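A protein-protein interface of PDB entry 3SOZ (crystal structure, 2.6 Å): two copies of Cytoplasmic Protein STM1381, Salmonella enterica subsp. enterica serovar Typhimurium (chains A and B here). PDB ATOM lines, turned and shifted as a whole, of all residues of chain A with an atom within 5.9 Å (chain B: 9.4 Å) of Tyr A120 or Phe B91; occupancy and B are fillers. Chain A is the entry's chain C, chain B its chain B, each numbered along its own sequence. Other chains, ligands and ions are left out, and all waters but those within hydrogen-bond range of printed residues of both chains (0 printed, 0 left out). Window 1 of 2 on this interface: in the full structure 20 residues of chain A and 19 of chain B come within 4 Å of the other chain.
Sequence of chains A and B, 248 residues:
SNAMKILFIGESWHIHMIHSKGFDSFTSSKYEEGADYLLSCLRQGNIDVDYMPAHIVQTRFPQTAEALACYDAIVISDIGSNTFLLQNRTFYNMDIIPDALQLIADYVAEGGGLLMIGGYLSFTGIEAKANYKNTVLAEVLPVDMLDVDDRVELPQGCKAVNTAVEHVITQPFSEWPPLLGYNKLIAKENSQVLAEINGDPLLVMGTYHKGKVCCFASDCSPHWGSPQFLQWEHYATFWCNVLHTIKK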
ATOM      1  N   TRP A  13       9.530   2.827  -6.495  1.00  0.00           N
ATOM      2  CA  TRP A  13       8.406   3.546  -7.046  1.00  0.00           C
ATOM      3  C   TRP A  13       7.736   2.747  -8.124  1.00  0.00           C
ATOM      4  O   TRP A  13       8.386   2.098  -8.915  1.00  0.00           O
ATOM      5  CB  TRP A  13       8.929   4.756  -7.720  1.00  0.00           C
ATOM      6  CG  TRP A  13       9.360   5.763  -6.824  1.00  0.00           C
ATOM      7  CD1 TRP A  13      10.654   6.099  -6.545  1.00  0.00           C
ATOM      8  CD2 TRP A  13       8.516   6.691  -6.089  1.00  0.00           C
ATOM      9  NE1 TRP A  13      10.669   7.167  -5.668  1.00  0.00           N
ATOM     10  CE2 TRP A  13       9.378   7.550  -5.371  1.00  0.00           C
ATOM     11  CE3 TRP A  13       7.126   6.880  -5.986  1.00  0.00           C
ATOM     12  CZ2 TRP A  13       8.896   8.599  -4.551  1.00  0.00           C
ATOM     13  CZ3 TRP A  13       6.646   7.890  -5.164  1.00  0.00           C
ATOM     14  CH2 TRP A  13       7.551   8.765  -4.467  1.00  0.00           C
ATOM     15  N   ASP A  78      12.283   7.247   2.574  1.00  0.00           N
ATOM     16  CA  ASP A  78      11.427   7.925   1.568  1.00  0.00           C
ATOM     17  C   ASP A  78      10.150   7.126   1.406  1.00  0.00           C
ATOM     18  O   ASP A  78       9.788   6.710   0.283  1.00  0.00           O
ATOM     19  CB  ASP A  78      12.232   8.059   0.271  1.00  0.00           C
ATOM     20  CG  ASP A  78      11.461   8.695  -0.882  1.00  0.00           C
ATOM     21  OD1 ASP A  78      10.736   9.723  -0.701  1.00  0.00           O
ATOM     22  OD2 ASP A  78      11.657   8.160  -2.003  1.00  0.00           O
ATOM     23  N   GLY A 118      15.828  11.195   3.496  1.00  0.00           N
ATOM     24  CA  GLY A 118      14.904  12.122   2.863  1.00  0.00           C
ATOM     25  C   GLY A 118      14.589  11.637   1.452  1.00  0.00           C
ATOM     26  O   GLY A 118      15.154  10.608   0.971  1.00  0.00           O
ATOM     27  N   GLY A 119      13.692  12.405   0.812  1.00  0.00           N
ATOM     28  CA  GLY A 119      13.140  12.106  -0.503  1.00  0.00           C
ATOM     29  C   GLY A 119      11.799  12.810  -0.525  1.00  0.00           C
ATOM     30  O   GLY A 119      11.464  13.545   0.388  1.00  0.00           O
ATOM     31  N   TYR A 120      11.013  12.554  -1.565  1.00  0.00           N
ATOM     32  CA  TYR A 120       9.752  13.228  -1.789  1.00  0.00           C
ATOM     33  C   TYR A 120       8.769  12.698  -0.764  1.00  0.00           C
ATOM     34  O   TYR A 120       7.810  13.400  -0.441  1.00  0.00           O
ATOM     35  CB  TYR A 120       9.266  12.950  -3.221  1.00  0.00           C
ATOM     36  CG  TYR A 120       9.844  13.859  -4.288  1.00  0.00           C
ATOM     37  CD1 TYR A 120      10.830  14.784  -3.971  1.00  0.00           C
ATOM     38  CD2 TYR A 120       9.406  13.795  -5.636  1.00  0.00           C
ATOM     39  CE1 TYR A 120      11.330  15.624  -4.885  1.00  0.00           C
ATOM     40  CE2 TYR A 120       9.944  14.645  -6.607  1.00  0.00           C
ATOM     41  CZ  TYR A 120      10.922  15.565  -6.201  1.00  0.00           C
ATOM     42  OH  TYR A 120      11.560  16.451  -7.086  1.00  0.00           O
ATOM     43  N   LEU A 121       9.012  11.489  -0.248  1.00  0.00           N
ATOM     44  CA  LEU A 121       8.096  10.934   0.762  1.00  0.00           C
ATOM     45  C   LEU A 121       8.648  10.853   2.228  1.00  0.00           C
ATOM     46  O   LEU A 121       8.111  10.056   3.069  1.00  0.00           O
ATOM     47  CB  LEU A 121       7.509   9.575   0.320  1.00  0.00           C
ATOM     48  CG  LEU A 121       6.541   9.642  -0.879  1.00  0.00           C
ATOM     49  CD1 LEU A 121       6.041   8.287  -1.112  1.00  0.00           C
ATOM     50  CD2 LEU A 121       5.343  10.608  -0.694  1.00  0.00           C
ATOM     51  N   SER A 122       9.692  11.679   2.513  1.00  0.00           N
ATOM     52  CA  SER A 122      10.224  11.822   3.869  1.00  0.00           C
ATOM     53  C   SER A 122       9.853  13.196   4.482  1.00  0.00           C
ATOM     54  O   SER A 122       9.602  14.196   3.733  1.00  0.00           O
ATOM     55  CB  SER A 122      11.714  11.647   3.903  1.00  0.00           C
ATOM     56  OG  SER A 122      12.116  10.374   3.451  1.00  0.00           O
ATOM     57  N   THR A 124       8.423  16.401   5.545  1.00  0.00           N
ATOM     58  CA  THR A 124       7.119  16.885   5.142  1.00  0.00           C
ATOM     59  C   THR A 124       6.718  16.382   3.756  1.00  0.00           C
ATOM     60  O   THR A 124       5.592  15.910   3.577  1.00  0.00           O
ATOM     61  CB  THR A 124       6.910  18.384   5.375  1.00  0.00           C
ATOM     62  OG1 THR A 124       6.939  18.584   6.788  1.00  0.00           O
ATOM     63  CG2 THR A 124       5.509  18.882   4.808  1.00  0.00           C
ATOM     64  N   GLY A 125       7.664  16.400   2.827  1.00  0.00           N
ATOM     65  CA  GLY A 125       7.505  15.705   1.576  1.00  0.00           C
ATOM     66  C   GLY A 125       6.911  16.577   0.487  1.00  0.00           C
ATOM     67  O   GLY A 125       6.279  17.611   0.776  1.00  0.00           O
ATOM     68  N   ILE A 126       7.081  16.172  -0.768  1.00  0.00           N
ATOM     69  CA  ILE A 126       6.386  16.836  -1.859  1.00  0.00           C
ATOM     70  C   ILE A 126       4.894  17.052  -1.587  1.00  0.00           C
ATOM     71  O   ILE A 126       4.169  16.126  -1.162  1.00  0.00           O
ATOM     72  CB  ILE A 126       6.613  16.108  -3.206  1.00  0.00           C
ATOM     73  CG1 ILE A 126       6.066  16.972  -4.347  1.00  0.00           C
ATOM     74  CG2 ILE A 126       5.957  14.765  -3.192  1.00  0.00           C
ATOM     75  CD1 ILE A 126       6.831  16.829  -5.647  1.00  0.00           C
ATOM     76  N   LYS A 129       3.012  15.707   1.589  1.00  0.00           N
ATOM     77  CA  LYS A 129       2.365  14.406   1.549  1.00  0.00           C
ATOM     78  C   LYS A 129       2.885  13.381   2.582  1.00  0.00           C
ATOM     79  O   LYS A 129       2.093  12.513   3.065  1.00  0.00           O
ATOM     80  CB  LYS A 129       2.550  13.786   0.162  1.00  0.00           C
ATOM     81  CG  LYS A 129       1.467  14.110  -0.801  1.00  0.00           C
ATOM     82  CD  LYS A 129       1.770  13.664  -2.239  1.00  0.00           C
ATOM     83  CE  LYS A 129       0.633  14.050  -3.230  1.00  0.00           C
ATOM     84  NZ  LYS A 129      -0.450  12.967  -3.197  1.00  0.00           N
ATOM     85  N   ALA A 130       4.195  13.444   2.858  1.00  0.00           N
ATOM     86  CA  ALA A 130       4.866  12.505   3.763  1.00  0.00           C
ATOM     87  C   ALA A 130       4.386  12.787   5.168  1.00  0.00           C
ATOM     88  O   ALA A 130       4.165  11.849   5.936  1.00  0.00           O
ATOM     89  CB  ALA A 130       6.401  12.633   3.677  1.00  0.00           C
ATOM     90  N   ARG A 151      10.582  20.450  -0.085  1.00  0.00           N
ATOM     91  CA  ARG A 151      11.644  20.243  -1.010  1.00  0.00           C
ATOM     92  C   ARG A 151      12.475  21.509  -1.230  1.00  0.00           C
ATOM     93  O   ARG A 151      11.942  22.617  -1.353  1.00  0.00           O
ATOM     94  CB  ARG A 151      11.085  19.729  -2.343  1.00  0.00           C
ATOM     95  CG  ARG A 151      10.267  18.407  -2.274  1.00  0.00           C
ATOM     96  CD  ARG A 151       8.944  18.618  -3.039  1.00  0.00           C
ATOM     97  NE  ARG A 151       9.276  18.809  -4.418  1.00  0.00           N
ATOM     98  CZ  ARG A 151       8.744  19.664  -5.280  1.00  0.00           C
ATOM     99  NH1 ARG A 151       7.710  20.461  -4.989  1.00  0.00           N
ATOM    100  NH2 ARG A 151       9.271  19.650  -6.480  1.00  0.00           N
ATOM    101  N   GLU A 153      14.784  22.252  -4.316  1.00  0.00           N
ATOM    102  CA  GLU A 153      15.353  21.622  -5.518  1.00  0.00           C
ATOM    103  C   GLU A 153      16.607  22.394  -5.973  1.00  0.00           C
ATOM    104  O   GLU A 153      16.650  23.643  -5.983  1.00  0.00           O
ATOM    105  CB  GLU A 153      14.336  21.465  -6.635  1.00  0.00           C
ATOM    106  CG  GLU A 153      13.014  20.844  -6.278  1.00  0.00           C
ATOM    107  CD  GLU A 153      12.984  19.326  -6.346  1.00  0.00           C
ATOM    108  OE1 GLU A 153      14.026  18.653  -6.521  1.00  0.00           O
ATOM    109  OE2 GLU A 153      11.856  18.784  -6.235  1.00  0.00           O
ATOM    110  N   ASN A 183      15.246  17.762   1.756  1.00  0.00           N
ATOM    111  CA  ASN A 183      14.170  18.292   2.587  1.00  0.00           C
ATOM    112  C   ASN A 183      14.660  19.447   3.499  1.00  0.00           C
ATOM    113  O   ASN A 183      15.668  19.313   4.162  1.00  0.00           O
ATOM    114  CB  ASN A 183      13.593  17.166   3.432  1.00  0.00           C
ATOM    115  CG  ASN A 183      12.981  16.046   2.588  1.00  0.00           C
ATOM    116  OD1 ASN A 183      13.647  15.039   2.275  1.00  0.00           O
ATOM    117  ND2 ASN A 183      11.708  16.203   2.234  1.00  0.00           N
ATOM    118  N   ASP A 219      18.471  12.261  -0.439  1.00  0.00           N
ATOM    119  CA  ASP A 219      18.064  10.905  -0.777  1.00  0.00           C
ATOM    120  C   ASP A 219      19.326  10.056  -0.946  1.00  0.00           C
ATOM    121  O   ASP A 219      20.412  10.585  -1.178  1.00  0.00           O
ATOM    122  CB  ASP A 219      17.206  10.911  -2.068  1.00  0.00           C
ATOM    123  CG  ASP A 219      16.286   9.677  -2.186  1.00  0.00           C
ATOM    124  OD1 ASP A 219      16.685   8.557  -1.739  1.00  0.00           O
ATOM    125  OD2 ASP A 219      15.148   9.835  -2.712  1.00  0.00           O
ATOM    126  N   HIS A 223      16.154  11.064  -7.594  1.00  0.00           N
ATOM    127  CA  HIS A 223      17.067  11.871  -8.398  1.00  0.00           C
ATOM    128  C   HIS A 223      17.919  12.872  -7.624  1.00  0.00           C
ATOM    129  O   HIS A 223      18.806  13.492  -8.226  1.00  0.00           O
ATOM    130  CB  HIS A 223      16.268  12.592  -9.463  1.00  0.00           C
ATOM    131  CG  HIS A 223      15.750  13.933  -9.052  1.00  0.00           C
ATOM    132  ND1 HIS A 223      14.500  14.104  -8.484  1.00  0.00           N
ATOM    133  CD2 HIS A 223      16.296  15.173  -9.175  1.00  0.00           C
ATOM    134  CE1 HIS A 223      14.314  15.394  -8.260  1.00  0.00           C
ATOM    135  NE2 HIS A 223      15.387  16.063  -8.673  1.00  0.00           N
ATOM    136  N   TRP A 224      17.628  13.078  -6.326  1.00  0.00           N
ATOM    137  CA  TRP A 224      18.457  13.938  -5.470  1.00  0.00           C
ATOM    138  C   TRP A 224      19.819  13.307  -5.240  1.00  0.00           C
ATOM    139  O   TRP A 224      20.879  13.997  -5.239  1.00  0.00           O
ATOM    140  CB  TRP A 224      17.792  14.172  -4.140  1.00  0.00           C
ATOM    141  CG  TRP A 224      16.625  15.150  -4.206  1.00  0.00           C
ATOM    142  CD1 TRP A 224      16.284  15.926  -5.262  1.00  0.00           C
ATOM    143  CD2 TRP A 224      15.732  15.498  -3.151  1.00  0.00           C
ATOM    144  NE1 TRP A 224      15.224  16.709  -4.951  1.00  0.00           N
ATOM    145  CE2 TRP A 224      14.848  16.457  -3.662  1.00  0.00           C
ATOM    146  CE3 TRP A 224      15.583  15.073  -1.830  1.00  0.00           C
ATOM    147  CZ2 TRP A 224      13.835  17.042  -2.897  1.00  0.00           C
ATOM    148  CZ3 TRP A 224      14.592  15.629  -1.065  1.00  0.00           C
ATOM    149  CH2 TRP A 224      13.728  16.624  -1.598  1.00  0.00           C
ATOM    150  N   GLN B  58      10.512  22.760 -20.357  1.00  0.00           N
ATOM    151  CA  GLN B  58      10.949  21.473 -19.876  1.00  0.00           C
ATOM    152  C   GLN B  58      12.140  20.857 -20.632  1.00  0.00           C
ATOM    153  O   GLN B  58      12.809  19.974 -20.098  1.00  0.00           O
ATOM    154  CB  GLN B  58       9.783  20.482 -19.886  1.00  0.00           C
ATOM    155  CG  GLN B  58       8.800  20.637 -18.747  1.00  0.00           C
ATOM    156  CD  GLN B  58       7.633  19.710 -18.880  1.00  0.00           C
ATOM    157  OE1 GLN B  58       7.175  19.471 -19.990  1.00  0.00           O
ATOM    158  NE2 GLN B  58       7.113  19.191 -17.751  1.00  0.00           N
ATOM    159  N   ASN B  82       7.546  23.927 -10.374  1.00  0.00           N
ATOM    160  CA  ASN B  82       8.042  22.586 -10.586  1.00  0.00           C
ATOM    161  C   ASN B  82       8.501  22.478 -12.030  1.00  0.00           C
ATOM    162  O   ASN B  82       9.575  21.900 -12.309  1.00  0.00           O
ATOM    163  CB  ASN B  82       6.942  21.591 -10.395  1.00  0.00           C
ATOM    164  CG  ASN B  82       6.675  21.221  -8.928  1.00  0.00           C
ATOM    165  OD1 ASN B  82       7.530  21.358  -8.065  1.00  0.00           O
ATOM    166  ND2 ASN B  82       5.479  20.650  -8.676  1.00  0.00           N
ATOM    167  N   THR B  83       7.724  23.109 -12.932  1.00  0.00           N
ATOM    168  CA  THR B  83       7.989  23.073 -14.344  1.00  0.00           C
ATOM    169  C   THR B  83       9.334  23.673 -14.662  1.00  0.00           C
ATOM    170  O   THR B  83      10.004  23.209 -15.576  1.00  0.00           O
ATOM    171  CB  THR B  83       6.886  23.750 -15.203  1.00  0.00           C
ATOM    172  OG1 THR B  83       5.748  22.888 -15.236  1.00  0.00           O
ATOM    173  CG2 THR B  83       7.366  23.897 -16.631  1.00  0.00           C
ATOM    174  N   PHE B  84       9.720  24.703 -13.930  1.00  0.00           N
ATOM    175  CA  PHE B  84      11.008  25.379 -14.162  1.00  0.00           C
ATOM    176  C   PHE B  84      12.164  24.684 -13.450  1.00  0.00           C
ATOM    177  O   PHE B  84      13.282  24.714 -13.928  1.00  0.00           O
ATOM    178  CB  PHE B  84      10.962  26.784 -13.597  1.00  0.00           C
ATOM    179  CG  PHE B  84      10.195  27.761 -14.413  1.00  0.00           C
ATOM    180  CD1 PHE B  84      10.831  28.449 -15.472  1.00  0.00           C
ATOM    181  CD2 PHE B  84       8.871  28.071 -14.075  1.00  0.00           C
ATOM    182  CE1 PHE B  84      10.149  29.387 -16.209  1.00  0.00           C
ATOM    183  CE2 PHE B  84       8.168  29.000 -14.813  1.00  0.00           C
ATOM    184  CZ  PHE B  84       8.809  29.680 -15.885  1.00  0.00           C
ATOM    185  N   LEU B  85      11.881  24.113 -12.272  1.00  0.00           N
ATOM    186  CA  LEU B  85      12.926  23.507 -11.443  1.00  0.00           C
ATOM    187  C   LEU B  85      13.164  22.007 -11.747  1.00  0.00           C
ATOM    188  O   LEU B  85      14.234  21.465 -11.439  1.00  0.00           O
ATOM    189  CB  LEU B  85      12.596  23.680  -9.949  1.00  0.00           C
ATOM    190  CG  LEU B  85      12.676  25.095  -9.343  1.00  0.00           C
ATOM    191  CD1 LEU B  85      12.053  25.132  -7.951  1.00  0.00           C
ATOM    192  CD2 LEU B  85      14.129  25.650  -9.331  1.00  0.00           C
ATOM    193  N   LEU B  86      12.149  21.340 -12.307  1.00  0.00           N
ATOM    194  CA  LEU B  86      12.248  19.929 -12.566  1.00  0.00           C
ATOM    195  C   LEU B  86      12.226  19.660 -14.048  1.00  0.00           C
ATOM    196  O   LEU B  86      11.420  18.895 -14.548  1.00  0.00           O
ATOM    197  CB  LEU B  86      11.141  19.165 -11.810  1.00  0.00           C
ATOM    198  CG  LEU B  86      11.426  19.264 -10.300  1.00  0.00           C
ATOM    199  CD1 LEU B  86      10.398  18.509  -9.520  1.00  0.00           C
ATOM    200  CD2 LEU B  86      12.880  18.742  -9.997  1.00  0.00           C
ATOM    201  N   GLN B  87      13.115  20.288 -14.775  1.00  0.00           N
ATOM    202  CA  GLN B  87      13.122  20.092 -16.218  1.00  0.00           C
ATOM    203  C   GLN B  87      13.358  18.594 -16.559  1.00  0.00           C
ATOM    204  O   GLN B  87      13.817  17.834 -15.716  1.00  0.00           O
ATOM    205  CB  GLN B  87      14.196  21.015 -16.849  1.00  0.00           C
ATOM    206  CG  GLN B  87      13.851  22.479 -16.681  1.00  0.00           C
ATOM    207  CD  GLN B  87      15.024  23.386 -17.013  1.00  0.00           C
ATOM    208  OE1 GLN B  87      15.967  23.003 -17.696  1.00  0.00           O
ATOM    209  NE2 GLN B  87      14.965  24.588 -16.541  1.00  0.00           N
ATOM    210  N   ASN B  88      13.062  18.171 -17.773  1.00  0.00           N
ATOM    211  CA  ASN B  88      13.170  16.727 -18.081  1.00  0.00           C
ATOM    212  C   ASN B  88      14.593  16.155 -17.850  1.00  0.00           C
ATOM    213  O   ASN B  88      14.769  15.032 -17.342  1.00  0.00           O
ATOM    214  CB  ASN B  88      12.662  16.357 -19.488  1.00  0.00           C
ATOM    215  CG  ASN B  88      11.249  16.812 -19.759  1.00  0.00           C
ATOM    216  OD1 ASN B  88      10.813  16.793 -20.892  1.00  0.00           O
ATOM    217  ND2 ASN B  88      10.550  17.266 -18.753  1.00  0.00           N
ATOM    218  N   ARG B  89      15.599  16.916 -18.214  1.00  0.00           N
ATOM    219  CA  ARG B  89      16.918  16.431 -18.003  1.00  0.00           C
ATOM    220  C   ARG B  89      17.251  16.246 -16.505  1.00  0.00           C
ATOM    221  O   ARG B  89      18.032  15.344 -16.161  1.00  0.00           O
ATOM    222  CB  ARG B  89      17.927  17.363 -18.673  1.00  0.00           C
ATOM    223  CG  ARG B  89      18.275  17.023 -20.149  1.00  0.00           C
ATOM    224  CD  ARG B  89      19.151  18.162 -20.747  1.00  0.00           C
ATOM    225  NE  ARG B  89      18.378  19.422 -20.880  1.00  0.00           N
ATOM    226  CZ  ARG B  89      18.859  20.587 -21.347  1.00  0.00           C
ATOM    227  NH1 ARG B  89      20.136  20.691 -21.715  1.00  0.00           N
ATOM    228  NH2 ARG B  89      18.065  21.657 -21.436  1.00  0.00           N
ATOM    229  N   THR B  90      16.701  17.115 -15.631  1.00  0.00           N
ATOM    230  CA  THR B  90      16.970  17.062 -14.210  1.00  0.00           C
ATOM    231  C   THR B  90      16.191  15.908 -13.637  1.00  0.00           C
ATOM    232  O   THR B  90      16.729  15.053 -12.952  1.00  0.00           O
ATOM    233  CB  THR B  90      16.431  18.255 -13.531  1.00  0.00           C
ATOM    234  OG1 THR B  90      17.030  19.439 -14.077  1.00  0.00           O
ATOM    235  CG2 THR B  90      16.659  18.185 -11.984  1.00  0.00           C
ATOM    236  N   PHE B  91      14.909  15.870 -13.933  1.00  0.00           N
ATOM    237  CA  PHE B  91      14.037  14.919 -13.310  1.00  0.00           C
ATOM    238  C   PHE B  91      14.209  13.497 -13.813  1.00  0.00           C
ATOM    239  O   PHE B  91      14.142  12.576 -13.033  1.00  0.00           O
ATOM    240  CB  PHE B  91      12.594  15.393 -13.420  1.00  0.00           C
ATOM    241  CG  PHE B  91      11.704  14.768 -12.421  1.00  0.00           C
ATOM    242  CD1 PHE B  91      11.897  15.003 -11.072  1.00  0.00           C
ATOM    243  CD2 PHE B  91      10.684  13.906 -12.810  1.00  0.00           C
ATOM    244  CE1 PHE B  91      11.063  14.403 -10.127  1.00  0.00           C
ATOM    245  CE2 PHE B  91       9.861  13.280 -11.865  1.00  0.00           C
ATOM    246  CZ  PHE B  91      10.038  13.547 -10.530  1.00  0.00           C
ATOM    247  N   TYR B  92      14.442  13.312 -15.104  1.00  0.00           N
ATOM    248  CA  TYR B  92      14.514  11.974 -15.682  1.00  0.00           C
ATOM    249  C   TYR B  92      15.939  11.513 -16.019  1.00  0.00           C
ATOM    250  O   TYR B  92      16.168  10.327 -16.034  1.00  0.00           O
ATOM    251  CB  TYR B  92      13.597  11.837 -16.914  1.00  0.00           C
ATOM    252  CG  TYR B  92      12.180  12.200 -16.630  1.00  0.00           C
ATOM    253  CD1 TYR B  92      11.350  11.323 -15.917  1.00  0.00           C
ATOM    254  CD2 TYR B  92      11.663  13.463 -16.990  1.00  0.00           C
ATOM    255  CE1 TYR B  92      10.029  11.654 -15.622  1.00  0.00           C
ATOM    256  CE2 TYR B  92      10.331  13.799 -16.690  1.00  0.00           C
ATOM    257  CZ  TYR B  92       9.543  12.860 -16.013  1.00  0.00           C
ATOM    258  OH  TYR B  92       8.274  13.145 -15.673  1.00  0.00           O
ATOM    259  N   ASN B  93      16.882  12.415 -16.313  1.00  0.00           N
ATOM    260  CA  ASN B  93      18.279  11.974 -16.532  1.00  0.00           C
ATOM    261  C   ASN B  93      19.277  12.234 -15.440  1.00  0.00           C
ATOM    262  O   ASN B  93      20.274  11.548 -15.353  1.00  0.00           O
ATOM    263  CB  ASN B  93      18.852  12.489 -17.823  1.00  0.00           C
ATOM    264  CG  ASN B  93      18.007  12.110 -18.987  1.00  0.00           C
ATOM    265  OD1 ASN B  93      16.872  12.571 -19.106  1.00  0.00           O
ATOM    266  ND2 ASN B  93      18.542  11.280 -19.862  1.00  0.00           N
ATOM    267  N   MET B  94      19.017  13.204 -14.585  1.00  0.00           N
ATOM    268  CA  MET B  94      19.949  13.468 -13.494  1.00  0.00           C
ATOM    269  C   MET B  94      21.177  14.123 -14.110  1.00  0.00           C
ATOM    270  O   MET B  94      22.286  13.918 -13.654  1.00  0.00           O
ATOM    271  CB  MET B  94      20.395  12.147 -12.803  1.00  0.00           C
ATOM    272  CG  MET B  94      19.277  11.227 -12.163  1.00  0.00           C
ATOM    273  SD  MET B  94      19.812  10.791 -10.286  1.00  0.00           S
ATOM    274  CE  MET B  94      21.283   9.505 -10.700  1.00  0.00           C
ATOM    275  N   ASP B  95      20.984  14.868 -15.183  1.00  0.00           N
ATOM    276  CA  ASP B  95      22.002  15.765 -15.647  1.00  0.00           C
ATOM    277  C   ASP B  95      22.001  16.913 -14.679  1.00  0.00           C
ATOM    278  O   ASP B  95      21.008  17.118 -14.005  1.00  0.00           O
ATOM    279  CB  ASP B  95      21.624  16.292 -17.027  1.00  0.00           C
ATOM    280  CG  ASP B  95      21.850  15.282 -18.112  1.00  0.00           C
ATOM    281  OD1 ASP B  95      22.703  14.376 -17.879  1.00  0.00           O
ATOM    282  OD2 ASP B  95      21.177  15.410 -19.178  1.00  0.00           O
ATOM    283  N   ILE B  96      23.087  17.673 -14.628  1.00  0.00           N
ATOM    284  CA  ILE B  96      23.194  18.845 -13.785  1.00  0.00           C
ATOM    285  C   ILE B  96      22.970  20.061 -14.659  1.00  0.00           C
ATOM    286  O   ILE B  96      23.699  20.264 -15.601  1.00  0.00           O
ATOM    287  CB  ILE B  96      24.598  18.873 -13.084  1.00  0.00           C
ATOM    288  CG1 ILE B  96      24.514  18.253 -11.710  1.00  0.00           C
ATOM    289  CG2 ILE B  96      25.188  20.280 -12.947  1.00  0.00           C
ATOM    290  CD1 ILE B  96      25.834  17.664 -11.265  1.00  0.00           C
ATOM    291  N   ILE B  97      22.015  20.901 -14.282  1.00  0.00           N
ATOM    292  CA  ILE B  97      21.410  21.928 -15.125  1.00  0.00           C
ATOM    293  C   ILE B  97      21.288  23.217 -14.302  1.00  0.00           C
ATOM    294  O   ILE B  97      21.031  23.149 -13.122  1.00  0.00           O
ATOM    295  CB  ILE B  97      19.970  21.390 -15.532  1.00  0.00           C
ATOM    296  CG1 ILE B  97      20.093  20.401 -16.667  1.00  0.00           C
ATOM    297  CG2 ILE B  97      18.942  22.452 -15.932  1.00  0.00           C
ATOM    298  CD1 ILE B  97      18.817  19.576 -16.791  1.00  0.00           C
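The side-chain amide oxygen of Asn B82 sits at hydrogen-bond distance from the guanidinium group of Arg A151, at 2.9 Å.
The backbone carbonyl oxygen of His A223 sits close to the side-chain sulfur of Met B94, at 3.5 Å.
Among the printed residues, pairs that only touch across the chains: Tyr A120 with Leu B86, Tyr A120 with Phe B91, Arg A151 with Leu B86, Glu A153 with Leu B86, His A223 with Leu B86, His A223 with Thr B90 and His A223 with Phe B91.
The backbone carbonyl oxygen (O) of Arg B89 sits at hydrogen-bond distance from the backbone NH (N) of Met B94, 2.8 Å away.
The side-chain carboxylate (OD1) of Asp A78 is in hydrogen-bond range of the backbone NH (N) of Tyr A120, 3.0 Å away.
The backbone carbonyl oxygen (O) of Tyr A120 lies within hydrogen-bond range of the backbone NH (N) of Ile A126 (2.9 Å).
The side-chain hydroxyl (OH) of Tyr A120 lies within hydrogen-bond range of the side-chain carboxylate (OE2) of Glu A153 (2.5 Å).
OE2 of Glu A153 lies within salt-bridge range of NH2 of Arg A151 (2.7 Å).
NE1 of Trp A224 is in hydrogen-bond range of OE1 of Glu A153, at 2.8 Å.
No residue of chain B comes within 4 Å of Gly A119.
Tyr A120 touches just these residues of chain B: Leu B86 (3.4 Å) and Phe B91 (3.7 Å).
No residue of chain B comes within 4 Å of Leu A121.
No residue of chain B comes within 4 Å of Ile A126.
Of the printed residues of chain B, Arg A151 touches Asn B82 and Leu B86.
Of the printed residues of chain A, Asn B82 touches Arg A151 (2.9 Å).
Phe B84 touches none of the printed residues of chain A.
Of the printed residues of chain A, Leu B86 touches Tyr A120 (3.4 Å), Arg A151 (3.4 Å), Glu A153 (3.6 Å) and His A223 (3.9 Å).
Of the printed residues of chain A, Thr B90 touches His A223 (3.8 Å).
Phe B91 touches two residues of chain A.
The nearest residue of chain B that does not touch Tyr A120 is Asn B82 (6.4 Å).
The nearest printed residue of chain A that does not touch Phe B91 is Glu A153 (5.9 Å).
The nearest printed residue of chain B that does not touch Arg A151 is Leu B85 (6.3 Å).
Printed residues of chain B that touch a printed residue of chain A: Asn B82, Leu B86, Thr B90, Phe B91 and Met B94.
Hydrophobic or aromatic side chains of chain B that line the printed part of chain A: Leu B86, Phe B91 and Met B94.
Along chain A the printed residues that touch a printed residue of chain B span positions 120 to 223.
Among the printed residues, 9 pairs touch across the chains.
Among the printed residues, no Asp or Glu carboxylate lies within 4 Å of a Lys or Arg side-chain nitrogen of the other chain.
No position is printed for both chains.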
